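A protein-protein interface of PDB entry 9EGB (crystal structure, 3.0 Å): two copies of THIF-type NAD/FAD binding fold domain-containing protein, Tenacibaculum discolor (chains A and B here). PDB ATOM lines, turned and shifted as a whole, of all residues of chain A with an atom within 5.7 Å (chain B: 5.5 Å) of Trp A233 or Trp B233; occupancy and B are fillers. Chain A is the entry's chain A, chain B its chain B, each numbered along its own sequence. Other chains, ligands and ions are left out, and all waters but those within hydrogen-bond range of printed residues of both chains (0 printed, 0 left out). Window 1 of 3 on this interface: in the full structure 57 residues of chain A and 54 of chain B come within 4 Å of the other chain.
The backbone carbonyl oxygen (O) of Gln A79 lies within hydrogen-bond range of the guanidinium group (NH1) of Arg B57.
The side-chain hydroxyl (OG) of Ser A229 sits at hydrogen-bond distance from the backbone carbonyl oxygen (O) of Cys B54, 2.7 Å away.
O of Cys A54 is in hydrogen-bond range of OG of Ser B229 (2.9 Å).
The guanidinium group of Arg A57 lies within hydrogen-bond range of the backbone carbonyl oxygen of Gln B79 (2.8 Å).
NE of Arg B57 lies within salt-bridge range of OE1 of Glu B53 (3.1 Å).
NE of Arg A57 lies within salt-bridge range of OE1 of Glu A53, at 2.9 Å.
SG of Cys B54 is in hydrogen-bond range of O of Ala B236, at 3.7 Å.
The side-chain amide nitrogen of Gln A79 lies close to the guanidinium group of Arg A78 (3.4 Å).
The side-chain amide nitrogen of Gln B79 sits close to the guanidinium group of Arg B78 (3.5 Å).
Ile A50 touches Trp B233.
Trp B233 touches Glu A53.
Cys A54 touches Trp B233.
CD of Arg A57 touches CH2 of Trp B233, at 3.5 Å.
Gly B237 touches Val A230 (O to CB, 3.6 Å).
Trp A233 touches Glu B53.
Cys B54 touches Trp A233 (SG to CG, 3.8 Å).
Arg B57 touches Trp A233.
CB of Ala B236 touches CD1 of Trp A233, 3.6 Å away.
Gly A237 touches Val B230.
Leu A228 touches none of the printed residues of chain B.
Gly A231 touches none of the printed residues of chain B.
Printed residues of chain B within 4 Å of Trp A233: Ile B50 (3.6 Å), Glu B53 (3.4 Å), Cys B54 (3.8 Å), Arg B57 (3.7 Å), Trp B233 (3.4 Å) and Ala B236 (3.6 Å).
Printed residues of chain A within 4 Å of Ile B50: Trp A233.
Of the printed residues of chain A, Ala B236 touches Trp A233 (3.6 Å).
Of the printed residues of chain A, Gly B237 touches Val A230 (3.6 Å).
The nearest residue of chain B that does not touch Trp A233 is Gly B237 (4.2 Å).
The nearest printed residue of chain A that does not touch Arg B57 is Ser A229 (4.1 Å).
Of the 17 printed residues of chain B, 10 touch a printed residue of chain A.
Hydrophobic or aromatic side chains of chain B that line the printed part of chain A: Ile B50, Val B230, Trp B233 and Ala B236.
Hydrophobic or aromatic side chains of chain A within 4 Å of the printed part of chain B: Ile A50, Val A230, Trp A233 and Ala A236.
Along chain A the printed residues that touch a printed residue of chain B span positions 50 to 237.
Among the printed residues, no Asp or Glu carboxylate lies within 4 Å of a Lys or Arg side-chain nitrogen of the other chain.
Glu A53 touches Trp B233, and with the chains exchanged Trp A233 touches Glu B53.
Cys A54 touches Ser B229, and with the chains exchanged Ser A229 touches Cys B54.
Cys A54 touches Trp B233, and with the chains exchanged Trp A233 touches Cys B54.
Arg A57 touches Gln B79, and with the chains exchanged Gln A79 touches Arg B57.
Positions printed for both chains: 50, 53, 54, 57, 78, 79, 228, 229, 230, 231, 232, 233, 234, 235, 236, 237 and 238.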
ATOM      1  N   ILE A  50     -31.357  -1.339 -22.862  1.00  0.00           N
ATOM      2  CA  ILE A  50     -30.488  -1.087 -21.711  1.00  0.00           C
ATOM      3  C   ILE A  50     -29.187  -0.444 -22.157  1.00  0.00           C
ATOM      4  O   ILE A  50     -28.727   0.536 -21.553  1.00  0.00           O
ATOM      5  CB  ILE A  50     -30.214  -2.372 -20.903  1.00  0.00           C
ATOM      6  CG1 ILE A  50     -31.491  -3.112 -20.549  1.00  0.00           C
ATOM      7  CG2 ILE A  50     -29.550  -2.028 -19.605  1.00  0.00           C
ATOM      8  CD1 ILE A  50     -32.394  -2.275 -19.648  1.00  0.00           C
ATOM      9  N   GLU A  53     -29.572   3.434 -22.862  1.00  0.00           N
ATOM     10  CA  GLU A  53     -29.658   4.356 -21.733  1.00  0.00           C
ATOM     11  C   GLU A  53     -28.292   4.580 -21.099  1.00  0.00           C
ATOM     12  O   GLU A  53     -27.891   5.724 -20.855  1.00  0.00           O
ATOM     13  CB  GLU A  53     -30.653   3.855 -20.681  1.00  0.00           C
ATOM     14  CG  GLU A  53     -30.627   4.719 -19.398  1.00  0.00           C
ATOM     15  CD  GLU A  53     -31.834   4.541 -18.484  1.00  0.00           C
ATOM     16  OE1 GLU A  53     -31.713   4.852 -17.282  1.00  0.00           O
ATOM     17  OE2 GLU A  53     -32.913   4.138 -18.959  1.00  0.00           O
ATOM     18  N   CYS A  54     -27.561   3.497 -20.832  1.00  0.00           N
ATOM     19  CA  CYS A  54     -26.239   3.632 -20.228  1.00  0.00           C
ATOM     20  C   CYS A  54     -25.312   4.456 -21.111  1.00  0.00           C
ATOM     21  O   CYS A  54     -24.519   5.262 -20.616  1.00  0.00           O
ATOM     22  CB  CYS A  54     -25.644   2.255 -19.970  1.00  0.00           C
ATOM     23  SG  CYS A  54     -24.087   2.317 -19.087  1.00  0.00           S
ATOM     24  N   ARG A  57     -26.593   8.232 -21.027  1.00  0.00           N
ATOM     25  CA  ARG A  57     -26.200   8.885 -19.786  1.00  0.00           C
ATOM     26  C   ARG A  57     -24.697   9.116 -19.721  1.00  0.00           C
ATOM     27  O   ARG A  57     -24.249  10.097 -19.120  1.00  0.00           O
ATOM     28  CB  ARG A  57     -26.678   8.077 -18.583  1.00  0.00           C
ATOM     29  CG  ARG A  57     -28.189   7.975 -18.423  1.00  0.00           C
ATOM     30  CD  ARG A  57     -28.499   7.298 -17.077  1.00  0.00           C
ATOM     31  NE  ARG A  57     -29.922   7.103 -16.803  1.00  0.00           N
ATOM     32  CZ  ARG A  57     -30.723   8.051 -16.308  1.00  0.00           C
ATOM     33  NH1 ARG A  57     -30.246   9.261 -16.046  1.00  0.00           N
ATOM     34  NH2 ARG A  57     -32.008   7.801 -16.084  1.00  0.00           N
ATOM     35  N   ARG A  78     -35.730  -7.865 -18.044  1.00  0.00           N
ATOM     36  CA  ARG A  78     -34.372  -7.572 -18.501  1.00  0.00           C
ATOM     37  C   ARG A  78     -34.258  -6.429 -19.510  1.00  0.00           C
ATOM     38  O   ARG A  78     -33.148  -6.084 -19.938  1.00  0.00           O
ATOM     39  CB  ARG A  78     -33.781  -8.823 -19.144  1.00  0.00           C
ATOM     40  CG  ARG A  78     -34.473  -9.160 -20.455  1.00  0.00           C
ATOM     41  CD  ARG A  78     -34.230 -10.591 -20.855  1.00  0.00           C
ATOM     42  NE  ARG A  78     -34.616 -10.861 -22.235  1.00  0.00           N
ATOM     43  CZ  ARG A  78     -35.869 -11.076 -22.625  1.00  0.00           C
ATOM     44  NH1 ARG A  78     -36.851 -11.057 -21.741  1.00  0.00           N
ATOM     45  NH2 ARG A  78     -36.146 -11.319 -23.896  1.00  0.00           N
ATOM     46  N   GLN A  79     -35.379  -5.837 -19.907  1.00  0.00           N
ATOM     47  CA  GLN A  79     -35.363  -4.791 -20.916  1.00  0.00           C
ATOM     48  C   GLN A  79     -35.963  -3.499 -20.389  1.00  0.00           C
ATOM     49  O   GLN A  79     -36.702  -3.482 -19.402  1.00  0.00           O
ATOM     50  CB  GLN A  79     -36.077  -5.228 -22.191  1.00  0.00           C
ATOM     51  CG  GLN A  79     -35.377  -6.404 -22.812  1.00  0.00           C
ATOM     52  CD  GLN A  79     -36.011  -6.878 -24.086  1.00  0.00           C
ATOM     53  OE1 GLN A  79     -36.861  -6.201 -24.674  1.00  0.00           O
ATOM     54  NE2 GLN A  79     -35.572  -8.040 -24.548  1.00  0.00           N
ATOM     55  N   LEU A 228     -31.335 -12.695 -17.849  1.00  0.00           N
ATOM     56  CA  LEU A 228     -31.576 -12.087 -16.538  1.00  0.00           C
ATOM     57  C   LEU A 228     -31.290 -10.595 -16.586  1.00  0.00           C
ATOM     58  O   LEU A 228     -30.580 -10.109 -17.472  1.00  0.00           O
ATOM     59  CB  LEU A 228     -30.716 -12.707 -15.426  1.00  0.00           C
ATOM     60  CG  LEU A 228     -30.814 -14.221 -15.271  1.00  0.00           C
ATOM     61  CD1 LEU A 228     -29.816 -14.724 -14.242  1.00  0.00           C
ATOM     62  CD2 LEU A 228     -32.241 -14.625 -14.933  1.00  0.00           C
ATOM     63  N   SER A 229     -31.871  -9.852 -15.639  1.00  0.00           N
ATOM     64  CA  SER A 229     -31.557  -8.425 -15.597  1.00  0.00           C
ATOM     65  C   SER A 229     -30.077  -8.182 -15.309  1.00  0.00           C
ATOM     66  O   SER A 229     -29.501  -7.217 -15.822  1.00  0.00           O
ATOM     67  CB  SER A 229     -32.415  -7.718 -14.543  1.00  0.00           C
ATOM     68  OG  SER A 229     -32.137  -8.204 -13.240  1.00  0.00           O
ATOM     69  N   VAL A 230     -29.439  -9.060 -14.523  1.00  0.00           N
ATOM     70  CA  VAL A 230     -28.045  -8.836 -14.134  1.00  0.00           C
ATOM     71  C   VAL A 230     -27.160  -8.800 -15.377  1.00  0.00           C
ATOM     72  O   VAL A 230     -26.312  -7.912 -15.537  1.00  0.00           O
ATOM     73  CB  VAL A 230     -27.582  -9.853 -13.064  1.00  0.00           C
ATOM     74  CG1 VAL A 230     -28.698 -10.810 -12.681  1.00  0.00           C
ATOM     75  CG2 VAL A 230     -26.306 -10.567 -13.441  1.00  0.00           C
ATOM     76  N   GLY A 231     -27.300  -9.800 -16.242  1.00  0.00           N
ATOM     77  CA  GLY A 231     -26.506  -9.829 -17.461  1.00  0.00           C
ATOM     78  C   GLY A 231     -26.796  -8.657 -18.382  1.00  0.00           C
ATOM     79  O   GLY A 231     -25.886  -8.135 -19.028  1.00  0.00           O
ATOM     80  N   SER A 232     -28.068  -8.236 -18.470  1.00  0.00           N
ATOM     81  CA  SER A 232     -28.400  -7.063 -19.277  1.00  0.00           C
ATOM     82  C   SER A 232     -27.671  -5.829 -18.769  1.00  0.00           C
ATOM     83  O   SER A 232     -27.036  -5.103 -19.545  1.00  0.00           O
ATOM     84  CB  SER A 232     -29.910  -6.801 -19.279  1.00  0.00           C
ATOM     85  OG  SER A 232     -30.583  -7.509 -20.303  1.00  0.00           O
ATOM     86  N   TRP A 233     -27.720  -5.600 -17.453  1.00  0.00           N
ATOM     87  CA  TRP A 233     -27.080  -4.421 -16.879  1.00  0.00           C
ATOM     88  C   TRP A 233     -25.565  -4.472 -17.013  1.00  0.00           C
ATOM     89  O   TRP A 233     -24.947  -3.468 -17.375  1.00  0.00           O
ATOM     90  CB  TRP A 233     -27.500  -4.252 -15.414  1.00  0.00           C
ATOM     91  CG  TRP A 233     -28.577  -3.195 -15.188  1.00  0.00           C
ATOM     92  CD1 TRP A 233     -28.402  -1.985 -14.583  1.00  0.00           C
ATOM     93  CD2 TRP A 233     -29.953  -3.233 -15.609  1.00  0.00           C
ATOM     94  NE1 TRP A 233     -29.579  -1.281 -14.574  1.00  0.00           N
ATOM     95  CE2 TRP A 233     -30.546  -2.019 -15.205  1.00  0.00           C
ATOM     96  CE3 TRP A 233     -30.738  -4.170 -16.286  1.00  0.00           C
ATOM     97  CZ2 TRP A 233     -31.892  -1.719 -15.445  1.00  0.00           C
ATOM     98  CZ3 TRP A 233     -32.070  -3.869 -16.532  1.00  0.00           C
ATOM     99  CH2 TRP A 233     -32.635  -2.654 -16.109  1.00  0.00           C
ATOM    100  N   VAL A 234     -24.955  -5.636 -16.791  1.00  0.00           N
ATOM    101  CA  VAL A 234     -23.508  -5.743 -16.937  1.00  0.00           C
ATOM    102  C   VAL A 234     -23.077  -5.537 -18.389  1.00  0.00           C
ATOM    103  O   VAL A 234     -22.092  -4.836 -18.666  1.00  0.00           O
ATOM    104  CB  VAL A 234     -23.022  -7.092 -16.387  1.00  0.00           C
ATOM    105  CG1 VAL A 234     -21.559  -7.315 -16.782  1.00  0.00           C
ATOM    106  CG2 VAL A 234     -23.211  -7.134 -14.885  1.00  0.00           C
ATOM    107  N   VAL A 235     -23.795  -6.142 -19.337  1.00  0.00           N
ATOM    108  CA  VAL A 235     -23.385  -6.033 -20.735  1.00  0.00           C
ATOM    109  C   VAL A 235     -23.566  -4.611 -21.251  1.00  0.00           C
ATOM    110  O   VAL A 235     -22.824  -4.173 -22.142  1.00  0.00           O
ATOM    111  CB  VAL A 235     -24.139  -7.056 -21.600  1.00  0.00           C
ATOM    112  CG1 VAL A 235     -25.487  -6.504 -22.037  1.00  0.00           C
ATOM    113  CG2 VAL A 235     -23.297  -7.440 -22.795  1.00  0.00           C
ATOM    114  N   ALA A 236     -24.559  -3.882 -20.721  1.00  0.00           N
ATOM    115  CA  ALA A 236     -24.749  -2.479 -21.080  1.00  0.00           C
ATOM    116  C   ALA A 236     -23.562  -1.633 -20.651  1.00  0.00           C
ATOM    117  O   ALA A 236     -23.130  -0.733 -21.388  1.00  0.00           O
ATOM    118  CB  ALA A 236     -26.028  -1.933 -20.454  1.00  0.00           C
ATOM    119  N   GLY A 237     -23.021  -1.910 -19.457  1.00  0.00           N
ATOM    120  CA  GLY A 237     -21.838  -1.198 -19.003  1.00  0.00           C
ATOM    121  C   GLY A 237     -20.639  -1.491 -19.876  1.00  0.00           C
ATOM    122  O   GLY A 237     -19.900  -0.579 -20.259  1.00  0.00           O
ATOM    123  N   MET A 238     -20.436  -2.769 -20.202  1.00  0.00           N
ATOM    124  CA  MET A 238     -19.323  -3.166 -21.058  1.00  0.00           C
ATOM    125  C   MET A 238     -19.388  -2.462 -22.404  1.00  0.00           C
ATOM    126  O   MET A 238     -18.380  -1.934 -22.891  1.00  0.00           O
ATOM    127  CB  MET A 238     -19.326  -4.676 -21.249  1.00  0.00           C
ATOM    128  CG  MET A 238     -19.245  -5.437 -19.965  1.00  0.00           C
ATOM    129  SD  MET A 238     -19.595  -7.170 -20.267  1.00  0.00           S
ATOM    130  CE  MET A 238     -18.096  -7.675 -21.103  1.00  0.00           C
ATOM    131  N   ILE B  50     -30.121   2.728  -9.539  1.00  0.00           N
ATOM    132  CA  ILE B  50     -29.806   1.776 -10.594  1.00  0.00           C
ATOM    133  C   ILE B  50     -29.934   0.354 -10.051  1.00  0.00           C
ATOM    134  O   ILE B  50     -30.451  -0.542 -10.729  1.00  0.00           O
ATOM    135  CB  ILE B  50     -28.407   2.045 -11.181  1.00  0.00           C
ATOM    136  CG1 ILE B  50     -28.208   3.531 -11.472  1.00  0.00           C
ATOM    137  CG2 ILE B  50     -28.254   1.311 -12.509  1.00  0.00           C
ATOM    138  CD1 ILE B  50     -29.143   4.080 -12.505  1.00  0.00           C
ATOM    139  N   GLU B  53     -33.776  -0.881  -9.769  1.00  0.00           N
ATOM    140  CA  GLU B  53     -34.454  -1.336 -10.985  1.00  0.00           C
ATOM    141  C   GLU B  53     -33.989  -2.722 -11.421  1.00  0.00           C
ATOM    142  O   GLU B  53     -34.809  -3.598 -11.735  1.00  0.00           O
ATOM    143  CB  GLU B  53     -34.259  -0.332 -12.119  1.00  0.00           C
ATOM    144  CG  GLU B  53     -34.782  -0.854 -13.450  1.00  0.00           C
ATOM    145  CD  GLU B  53     -34.910   0.215 -14.498  1.00  0.00           C
ATOM    146  OE1 GLU B  53     -34.931  -0.117 -15.710  1.00  0.00           O
ATOM    147  OE2 GLU B  53     -35.044   1.386 -14.092  1.00  0.00           O
ATOM    148  N   CYS B  54     -32.676  -2.944 -11.436  1.00  0.00           N
ATOM    149  CA  CYS B  54     -32.157  -4.240 -11.851  1.00  0.00           C
ATOM    150  C   CYS B  54     -32.654  -5.345 -10.924  1.00  0.00           C
ATOM    151  O   CYS B  54     -33.034  -6.433 -11.375  1.00  0.00           O
ATOM    152  CB  CYS B  54     -30.631  -4.169 -11.891  1.00  0.00           C
ATOM    153  SG  CYS B  54     -29.806  -5.594 -12.554  1.00  0.00           S
ATOM    154  N   ARG B  57     -36.590  -5.896 -11.580  1.00  0.00           N
ATOM    155  CA  ARG B  57     -36.880  -6.668 -12.776  1.00  0.00           C
ATOM    156  C   ARG B  57     -36.510  -8.130 -12.578  1.00  0.00           C
ATOM    157  O   ARG B  57     -37.210  -9.021 -13.067  1.00  0.00           O
ATOM    158  CB  ARG B  57     -36.132  -6.072 -13.963  1.00  0.00           C
ATOM    159  CG  ARG B  57     -36.599  -4.667 -14.314  1.00  0.00           C
ATOM    160  CD  ARG B  57     -35.974  -4.197 -15.601  1.00  0.00           C
ATOM    161  NE  ARG B  57     -36.370  -2.840 -15.945  1.00  0.00           N
ATOM    162  CZ  ARG B  57     -37.517  -2.531 -16.542  1.00  0.00           C
ATOM    163  NH1 ARG B  57     -38.386  -3.481 -16.843  1.00  0.00           N
ATOM    164  NH2 ARG B  57     -37.793  -1.271 -16.838  1.00  0.00           N
ATOM    165  N   ARG B  78     -25.502   8.975 -14.350  1.00  0.00           N
ATOM    166  CA  ARG B  78     -25.254   7.680 -13.709  1.00  0.00           C
ATOM    167  C   ARG B  78     -26.371   7.172 -12.794  1.00  0.00           C
ATOM    168  O   ARG B  78     -26.249   6.089 -12.205  1.00  0.00           O
ATOM    169  CB  ARG B  78     -23.977   7.774 -12.879  1.00  0.00           C
ATOM    170  CG  ARG B  78     -24.171   8.681 -11.679  1.00  0.00           C
ATOM    171  CD  ARG B  78     -22.860   9.126 -11.080  1.00  0.00           C
ATOM    172  NE  ARG B  78     -23.030   9.761  -9.773  1.00  0.00           N
ATOM    173  CZ  ARG B  78     -23.389  11.032  -9.628  1.00  0.00           C
ATOM    174  NH1 ARG B  78     -23.607  11.776 -10.699  1.00  0.00           N
ATOM    175  NH2 ARG B  78     -23.522  11.566  -8.423  1.00  0.00           N
ATOM    176  N   GLN B  79     -27.431   7.949 -12.611  1.00  0.00           N
ATOM    177  CA  GLN B  79     -28.509   7.579 -11.705  1.00  0.00           C
ATOM    178  C   GLN B  79     -29.843   7.484 -12.437  1.00  0.00           C
ATOM    179  O   GLN B  79     -30.025   8.044 -13.521  1.00  0.00           O
ATOM    180  CB  GLN B  79     -28.617   8.537 -10.513  1.00  0.00           C
ATOM    181  CG  GLN B  79     -27.390   8.540  -9.641  1.00  0.00           C
ATOM    182  CD  GLN B  79     -27.517   9.488  -8.477  1.00  0.00           C
ATOM    183  OE1 GLN B  79     -28.607   9.980  -8.172  1.00  0.00           O
ATOM    184  NE2 GLN B  79     -26.406   9.739  -7.801  1.00  0.00           N
ATOM    185  N   LEU B 228     -19.203   7.118 -13.150  1.00  0.00           N
ATOM    186  CA  LEU B 228     -19.568   6.951 -14.542  1.00  0.00           C
ATOM    187  C   LEU B 228     -20.794   6.052 -14.644  1.00  0.00           C
ATOM    188  O   LEU B 228     -21.048   5.230 -13.764  1.00  0.00           O
ATOM    189  CB  LEU B 228     -18.370   6.338 -15.265  1.00  0.00           C
ATOM    190  CG  LEU B 228     -17.371   7.347 -15.833  1.00  0.00           C
ATOM    191  CD1 LEU B 228     -16.170   6.617 -16.410  1.00  0.00           C
ATOM    192  CD2 LEU B 228     -17.972   8.308 -16.809  1.00  0.00           C
ATOM    193  N   SER B 229     -21.554   6.181 -15.733  1.00  0.00           N
ATOM    194  CA  SER B 229     -22.679   5.266 -15.912  1.00  0.00           C
ATOM    195  C   SER B 229     -22.224   3.813 -16.023  1.00  0.00           C
ATOM    196  O   SER B 229     -22.986   2.898 -15.686  1.00  0.00           O
ATOM    197  CB  SER B 229     -23.503   5.646 -17.139  1.00  0.00           C
ATOM    198  OG  SER B 229     -22.749   5.520 -18.325  1.00  0.00           O
ATOM    199  N   VAL B 230     -21.009   3.583 -16.533  1.00  0.00           N
ATOM    200  CA  VAL B 230     -20.490   2.223 -16.708  1.00  0.00           C
ATOM    201  C   VAL B 230     -20.472   1.465 -15.384  1.00  0.00           C
ATOM    202  O   VAL B 230     -21.038   0.372 -15.268  1.00  0.00           O
ATOM    203  CB  VAL B 230     -19.089   2.271 -17.344  1.00  0.00           C
ATOM    204  CG1 VAL B 230     -18.429   0.921 -17.273  1.00  0.00           C
ATOM    205  CG2 VAL B 230     -19.175   2.745 -18.794  1.00  0.00           C
ATOM    206  N   GLY B 231     -19.850   2.054 -14.358  1.00  0.00           N
ATOM    207  CA  GLY B 231     -19.753   1.390 -13.066  1.00  0.00           C
ATOM    208  C   GLY B 231     -21.107   1.200 -12.407  1.00  0.00           C
ATOM    209  O   GLY B 231     -21.357   0.171 -11.769  1.00  0.00           O
ATOM    210  N   SER B 232     -21.994   2.201 -12.544  1.00  0.00           N
ATOM    211  CA  SER B 232     -23.340   2.112 -11.983  1.00  0.00           C
ATOM    212  C   SER B 232     -24.100   0.928 -12.561  1.00  0.00           C
ATOM    213  O   SER B 232     -24.693   0.133 -11.822  1.00  0.00           O
ATOM    214  CB  SER B 232     -24.108   3.407 -12.279  1.00  0.00           C
ATOM    215  OG  SER B 232     -23.917   4.407 -11.292  1.00  0.00           O
ATOM    216  N   TRP B 233     -24.087   0.782 -13.884  1.00  0.00           N
ATOM    217  CA  TRP B 233     -24.806  -0.330 -14.492  1.00  0.00           C
ATOM    218  C   TRP B 233     -24.184  -1.663 -14.092  1.00  0.00           C
ATOM    219  O   TRP B 233     -24.900  -2.610 -13.752  1.00  0.00           O
ATOM    220  CB  TRP B 233     -24.844  -0.140 -16.001  1.00  0.00           C
ATOM    221  CG  TRP B 233     -26.144   0.417 -16.486  1.00  0.00           C
ATOM    222  CD1 TRP B 233     -27.097  -0.236 -17.228  1.00  0.00           C
ATOM    223  CD2 TRP B 233     -26.683   1.712 -16.195  1.00  0.00           C
ATOM    224  NE1 TRP B 233     -28.167   0.594 -17.463  1.00  0.00           N
ATOM    225  CE2 TRP B 233     -27.942   1.792 -16.832  1.00  0.00           C
ATOM    226  CE3 TRP B 233     -26.217   2.816 -15.473  1.00  0.00           C
ATOM    227  CZ2 TRP B 233     -28.742   2.936 -16.767  1.00  0.00           C
ATOM    228  CZ3 TRP B 233     -27.012   3.948 -15.409  1.00  0.00           C
ATOM    229  CH2 TRP B 233     -28.263   3.997 -16.053  1.00  0.00           C
ATOM    230  N   VAL B 234     -22.849  -1.727 -14.057  1.00  0.00           N
ATOM    231  CA  VAL B 234     -22.163  -2.950 -13.657  1.00  0.00           C
ATOM    232  C   VAL B 234     -22.443  -3.283 -12.200  1.00  0.00           C
ATOM    233  O   VAL B 234     -22.746  -4.427 -11.858  1.00  0.00           O
ATOM    234  CB  VAL B 234     -20.655  -2.806 -13.893  1.00  0.00           C
ATOM    235  CG1 VAL B 234     -19.918  -3.949 -13.241  1.00  0.00           C
ATOM    236  CG2 VAL B 234     -20.380  -2.756 -15.356  1.00  0.00           C
ATOM    237  N   VAL B 235     -22.360  -2.291 -11.319  1.00  0.00           N
ATOM    238  CA  VAL B 235     -22.529  -2.616  -9.909  1.00  0.00           C
ATOM    239  C   VAL B 235     -23.968  -3.037  -9.632  1.00  0.00           C
ATOM    240  O   VAL B 235     -24.218  -3.896  -8.771  1.00  0.00           O
ATOM    241  CB  VAL B 235     -22.054  -1.444  -9.025  1.00  0.00           C
ATOM    242  CG1 VAL B 235     -23.128  -0.443  -8.825  1.00  0.00           C
ATOM    243  CG2 VAL B 235     -21.610  -1.958  -7.692  1.00  0.00           C
ATOM    244  N   ALA B 236     -24.922  -2.496 -10.396  1.00  0.00           N
ATOM    245  CA  ALA B 236     -26.314  -2.900 -10.249  1.00  0.00           C
ATOM    246  C   ALA B 236     -26.495  -4.377 -10.566  1.00  0.00           C
ATOM    247  O   ALA B 236     -27.239  -5.086  -9.877  1.00  0.00           O
ATOM    248  CB  ALA B 236     -27.206  -2.049 -11.152  1.00  0.00           C
ATOM    249  N   GLY B 237     -25.836  -4.860 -11.615  1.00  0.00           N
ATOM    250  CA  GLY B 237     -25.900  -6.280 -11.903  1.00  0.00           C
ATOM    251  C   GLY B 237     -25.259  -7.115 -10.821  1.00  0.00           C
ATOM    252  O   GLY B 237     -25.819  -8.130 -10.397  1.00  0.00           O
ATOM    253  N   MET B 238     -24.093  -6.683 -10.336  1.00  0.00           N
ATOM    254  CA  MET B 238     -23.419  -7.416  -9.270  1.00  0.00           C
ATOM    255  C   MET B 238     -24.313  -7.520  -8.044  1.00  0.00           C
ATOM    256  O   MET B 238     -24.488  -8.605  -7.471  1.00  0.00           O
ATOM    257  CB  MET B 238     -22.087  -6.746  -8.917  1.00  0.00           C
ATOM    258  CG  MET B 238     -21.121  -6.619 -10.079  1.00  0.00           C
ATOM    259  SD  MET B 238     -19.732  -5.569  -9.673  1.00  0.00           S
ATOM    260  CE  MET B 238     -18.806  -6.642  -8.599  1.00  0.00           C
